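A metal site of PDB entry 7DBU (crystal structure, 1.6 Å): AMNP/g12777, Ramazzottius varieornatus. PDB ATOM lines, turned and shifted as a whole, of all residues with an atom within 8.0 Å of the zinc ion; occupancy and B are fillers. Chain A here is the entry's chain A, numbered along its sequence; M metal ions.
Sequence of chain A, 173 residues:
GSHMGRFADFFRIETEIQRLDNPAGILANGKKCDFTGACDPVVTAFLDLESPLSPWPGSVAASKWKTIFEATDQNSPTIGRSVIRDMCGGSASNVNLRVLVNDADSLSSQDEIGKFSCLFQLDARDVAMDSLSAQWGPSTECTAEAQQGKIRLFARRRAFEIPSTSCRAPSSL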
ATOM      1  N   LEU A  27      16.329  -6.655  -1.233  1.00  0.00           N
ATOM      2  CA  LEU A  27      16.346  -8.042  -0.696  1.00  0.00           C
ATOM      3  C   LEU A  27      17.639  -8.696  -1.186  1.00  0.00           C
ATOM      4  O   LEU A  27      18.402  -8.160  -2.029  1.00  0.00           O
ATOM      5  CB  LEU A  27      15.169  -8.859  -1.170  1.00  0.00           C
ATOM      6  CG  LEU A  27      13.794  -8.211  -1.069  1.00  0.00           C
ATOM      7  CD1 LEU A  27      12.852  -9.013  -1.926  1.00  0.00           C
ATOM      8  CD2 LEU A  27      13.397  -8.232   0.422  1.00  0.00           C
ATOM      9  N   CYS A  33      12.735  -4.249  -1.562  1.00  0.00           N
ATOM     10  CA  CYS A  33      11.676  -4.679  -0.638  1.00  0.00           C
ATOM     11  C   CYS A  33      10.289  -4.202  -1.121  1.00  0.00           C
ATOM     12  O   CYS A  33      10.149  -2.983  -1.316  1.00  0.00           O
ATOM     13  CB  CYS A  33      11.866  -4.133   0.754  1.00  0.00           C
ATOM     14  SG  CYS A  33      13.353  -4.791   1.570  1.00  0.00           S
ATOM     15  N   ASP A  34       9.327  -5.112  -1.253  1.00  0.00           N
ATOM     16  CA  ASP A  34       7.913  -4.784  -1.598  1.00  0.00           C
ATOM     17  C   ASP A  34       7.862  -3.958  -2.897  1.00  0.00           C
ATOM     18  O   ASP A  34       6.769  -3.307  -3.148  1.00  0.00           O
ATOM     19  CB  ASP A  34       7.287  -3.971  -0.462  1.00  0.00           C
ATOM     20  CG  ASP A  34       7.313  -4.667   0.887  1.00  0.00           C
ATOM     21  OD1 ASP A  34       7.339  -5.923   0.842  1.00  0.00           O
ATOM     22  OD2 ASP A  34       7.323  -3.956   1.952  1.00  0.00           O
ATOM     23  N   PHE A  35       8.941  -3.937  -3.705  1.00  0.00           N
ATOM     24  CA  PHE A  35       9.103  -3.070  -4.910  1.00  0.00           C
ATOM     25  C   PHE A  35       8.899  -1.586  -4.605  1.00  0.00           C
ATOM     26  O   PHE A  35       8.705  -0.832  -5.562  1.00  0.00           O
ATOM     27  CB  PHE A  35       8.192  -3.585  -6.028  1.00  0.00           C
ATOM     28  CG  PHE A  35       8.660  -4.906  -6.599  1.00  0.00           C
ATOM     29  CD1 PHE A  35       9.834  -4.984  -7.356  1.00  0.00           C
ATOM     30  CD2 PHE A  35       8.013  -6.090  -6.279  1.00  0.00           C
ATOM     31  CE1 PHE A  35      10.304  -6.203  -7.823  1.00  0.00           C
ATOM     32  CE2 PHE A  35       8.519  -7.315  -6.711  1.00  0.00           C
ATOM     33  CZ  PHE A  35       9.651  -7.370  -7.495  1.00  0.00           C
ATOM     34  N   THR A  36       9.109  -1.166  -3.350  1.00  0.00           N
ATOM     35  CA  THR A  36       9.098   0.244  -2.885  1.00  0.00           C
ATOM     36  C   THR A  36      10.464   0.675  -2.391  1.00  0.00           C
ATOM     37  O   THR A  36      10.819   1.847  -2.520  1.00  0.00           O
ATOM     38  CB  THR A  36       8.061   0.451  -1.775  1.00  0.00           C
ATOM     39  OG1 THR A  36       8.453  -0.353  -0.658  1.00  0.00           O
ATOM     40  CG2 THR A  36       6.664   0.132  -2.285  1.00  0.00           C
ATOM     41  N   ALA A  38      10.983   0.303   0.803  1.00  0.00           N
ATOM     42  CA  ALA A  38      10.532   0.672   2.154  1.00  0.00           C
ATOM     43  C   ALA A  38      10.462  -0.633   2.956  1.00  0.00           C
ATOM     44  O   ALA A  38       9.396  -1.211   3.075  1.00  0.00           O
ATOM     45  CB  ALA A  38       9.241   1.411   2.206  1.00  0.00           C
ATOM     46  N   CYS A  39      11.632  -1.119   3.393  1.00  0.00           N
ATOM     47  CA  CYS A  39      11.760  -2.482   3.974  1.00  0.00           C
ATOM     48  C   CYS A  39      11.119  -2.559   5.384  1.00  0.00           C
ATOM     49  O   CYS A  39      11.127  -1.517   6.096  1.00  0.00           O
ATOM     50  CB  CYS A  39      13.226  -2.907   4.089  1.00  0.00           C
ATOM     51  SG  CYS A  39      14.081  -3.069   2.517  1.00  0.00           S
ATOM     52  N   ASP A  40      10.657  -3.762   5.789  1.00  0.00           N
ATOM     53  CA  ASP A  40       9.964  -3.982   7.080  1.00  0.00           C
ATOM     54  C   ASP A  40      10.640  -5.141   7.785  1.00  0.00           C
ATOM     55  O   ASP A  40      10.121  -6.242   7.878  1.00  0.00           O
ATOM     56  CB  ASP A  40       8.474  -4.226   6.821  1.00  0.00           C
ATOM     57  CG  ASP A  40       7.810  -3.164   5.937  1.00  0.00           C
ATOM     58  OD1 ASP A  40       7.773  -2.011   6.376  1.00  0.00           O
ATOM     59  OD2 ASP A  40       7.392  -3.520   4.783  1.00  0.00           O
ATOM     60  N   PRO A  41      11.878  -4.954   8.284  1.00  0.00           N
ATOM     61  CA  PRO A  41      12.699  -6.078   8.729  1.00  0.00           C
ATOM     62  C   PRO A  41      12.223  -6.781   9.996  1.00  0.00           C
ATOM     63  O   PRO A  41      11.844  -6.155  10.953  1.00  0.00           O
ATOM     64  CB  PRO A  41      14.089  -5.492   8.921  1.00  0.00           C
ATOM     65  CG  PRO A  41      13.934  -3.973   8.980  1.00  0.00           C
ATOM     66  CD  PRO A  41      12.561  -3.673   8.447  1.00  0.00           C
ATOM     67  N   ALA A  71      10.733  -3.995  12.717  1.00  0.00           N
ATOM     68  CA  ALA A  71      10.418  -2.577  12.469  1.00  0.00           C
ATOM     69  C   ALA A  71       9.642  -2.530  11.176  1.00  0.00           C
ATOM     70  O   ALA A  71       9.819  -3.428  10.316  1.00  0.00           O
ATOM     71  CB  ALA A  71      11.638  -1.699  12.363  1.00  0.00           C
ATOM     72  N   THR A  72       8.875  -1.463  11.065  1.00  0.00           N
ATOM     73  CA  THR A  72       8.145  -1.095   9.842  1.00  0.00           C
ATOM     74  C   THR A  72       8.832   0.125   9.220  1.00  0.00           C
ATOM     75  O   THR A  72       9.066   1.074   9.930  1.00  0.00           O
ATOM     76  CB  THR A  72       6.666  -0.828  10.141  1.00  0.00           C
ATOM     77  OG1 THR A  72       6.058  -2.050  10.568  1.00  0.00           O
ATOM     78  CG2 THR A  72       5.975  -0.288   8.915  1.00  0.00           C
ATOM     79  N   ASP A  73       9.070   0.095   7.913  1.00  0.00           N
ATOM     80  CA  ASP A  73       9.611   1.248   7.146  1.00  0.00           C
ATOM     81  C   ASP A  73      10.925   1.724   7.757  1.00  0.00           C
ATOM     82  O   ASP A  73      11.027   2.960   8.026  1.00  0.00           O
ATOM     83  CB  ASP A  73       8.640   2.425   7.114  1.00  0.00           C
ATOM     84  CG  ASP A  73       7.394   2.149   6.304  1.00  0.00           C
ATOM     85  OD1 ASP A  73       7.460   1.291   5.386  1.00  0.00           O
ATOM     86  OD2 ASP A  73       6.380   2.776   6.605  1.00  0.00           O
ATOM     87  N   ASN A 102      14.008 -11.079   7.344  1.00  0.00           N
ATOM     88  CA  ASN A 102      12.964 -11.107   6.293  1.00  0.00           C
ATOM     89  C   ASN A 102      12.305  -9.745   6.277  1.00  0.00           C
ATOM     90  O   ASN A 102      12.295  -9.036   7.284  1.00  0.00           O
ATOM     91  CB  ASN A 102      11.890 -12.159   6.527  1.00  0.00           C
ATOM     92  CG  ASN A 102      12.381 -13.571   6.271  1.00  0.00           C
ATOM     93  OD1 ASN A 102      13.102 -13.833   5.307  1.00  0.00           O
ATOM     94  ND2 ASN A 102      12.042 -14.492   7.156  1.00  0.00           N
ATOM     95  N   ASP A 103      11.675  -9.452   5.160  1.00  0.00           N
ATOM     96  CA  ASP A 103      10.611  -8.432   5.189  1.00  0.00           C
ATOM     97  C   ASP A 103       9.339  -9.067   5.751  1.00  0.00           C
ATOM     98  O   ASP A 103       9.017 -10.191   5.372  1.00  0.00           O
ATOM     99  CB  ASP A 103      10.413  -7.863   3.787  1.00  0.00           C
ATOM    100  CG  ASP A 103       9.531  -6.623   3.770  1.00  0.00           C
ATOM    101  OD1 ASP A 103       8.315  -6.745   3.916  1.00  0.00           O
ATOM    102  OD2 ASP A 103      10.075  -5.525   3.600  1.00  0.00           O
ATOM    103  N   ALA A 104       8.579  -8.313   6.558  1.00  0.00           N
ATOM    104  CA  ALA A 104       7.329  -8.734   7.214  1.00  0.00           C
ATOM    105  C   ALA A 104       6.278  -9.167   6.202  1.00  0.00           C
ATOM    106  O   ALA A 104       5.447 -10.022   6.530  1.00  0.00           O
ATOM    107  CB  ALA A 104       6.841  -7.630   8.125  1.00  0.00           C
ATOM    108  N   ASP A 105       6.308  -8.618   4.988  1.00  0.00           N
ATOM    109  CA  ASP A 105       5.262  -8.863   3.966  1.00  0.00           C
ATOM    110  C   ASP A 105       5.567 -10.117   3.145  1.00  0.00           C
ATOM    111  O   ASP A 105       6.681 -10.252   2.600  1.00  0.00           O
ATOM    112  CB  ASP A 105       5.132  -7.643   3.049  1.00  0.00           C
ATOM    113  CG  ASP A 105       4.657  -6.407   3.801  1.00  0.00           C
ATOM    114  OD1 ASP A 105       3.446  -6.383   4.152  1.00  0.00           O
ATOM    115  OD2 ASP A 105       5.486  -5.505   4.041  1.00  0.00           O
ATOM    116  N   SER A 106       4.535 -10.941   2.904  1.00  0.00           N
ATOM    117  CA  SER A 106       4.651 -12.250   2.208  1.00  0.00           C
ATOM    118  C   SER A 106       5.810 -13.045   2.818  1.00  0.00           C
ATOM    119  O   SER A 106       6.747 -13.442   2.064  1.00  0.00           O
ATOM    120  CB  SER A 106       4.841 -12.095   0.741  1.00  0.00           C
ATOM    121  OG  SER A 106       3.729 -11.421   0.176  1.00  0.00           O
ATOM    122  N   GLN A 110       8.338 -13.852  -0.296  1.00  0.00           N
ATOM    123  CA  GLN A 110       9.329 -12.809  -0.687  1.00  0.00           C
ATOM    124  C   GLN A 110      10.725 -13.302  -0.289  1.00  0.00           C
ATOM    125  O   GLN A 110      10.873 -13.826   0.830  1.00  0.00           O
ATOM    126  CB  GLN A 110       8.957 -11.449  -0.067  1.00  0.00           C
ATOM    127  CG  GLN A 110       9.860 -10.286  -0.453  1.00  0.00           C
ATOM    128  CD  GLN A 110       9.235  -8.907  -0.335  1.00  0.00           C
ATOM    129  OE1 GLN A 110       9.673  -7.998  -1.006  1.00  0.00           O
ATOM    130  NE2 GLN A 110       8.277  -8.718   0.539  1.00  0.00           N
ATOM    131  N   ILE A 113      15.685 -10.517   3.176  1.00  0.00           N
ATOM    132  CA  ILE A 113      16.641  -9.395   3.165  1.00  0.00           C
ATOM    133  C   ILE A 113      18.063  -9.910   3.276  1.00  0.00           C
ATOM    134  O   ILE A 113      18.928  -9.520   2.494  1.00  0.00           O
ATOM    135  CB  ILE A 113      16.228  -8.312   4.194  1.00  0.00           C
ATOM    136  CG1 ILE A 113      14.946  -7.571   3.747  1.00  0.00           C
ATOM    137  CG2 ILE A 113      17.401  -7.367   4.383  1.00  0.00           C
ATOM    138  CD1 ILE A 113      14.312  -6.681   4.786  1.00  0.00           C
HETATM  139 ZN    ZN M   1       7.320  -5.075   3.585  1.00  0.00          ZN
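Along chain A the residues within 4 Å of the zinc ion span positions 34 to 105.
The side-chain carboxylate (OD2) of Asp 105 is bound to the zinc ion, at 1.9 Å. The zinc ion is bound by OD2 of Asp 40 (2.0 Å). The zinc ion is bound by OD1 of Asp 103 (2.0 Å). OD2 of Asp 34 binds the zinc ion. The zinc ion has four donor atoms within binding distance. Slightly farther from the zinc ion lies OD2 of Asp 103 (2.8 Å).
O of Asp 105 lies within hydrogen-bond range of NE2 of Gln 110, 3.0 Å away. The backbone NH of Ala 104 sits at hydrogen-bond distance from the backbone carbonyl oxygen of Asp 40 (2.9 Å). The side-chain carboxylate of Asp 40 lies within hydrogen-bond range of the backbone NH of Asp 73. The backbone NH of Asp 34 sits at hydrogen-bond distance from the side-chain amide oxygen of Gln 110 (2.9 Å). SG of Cys 39 is disulfide-bonded to SG of Cys 33.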
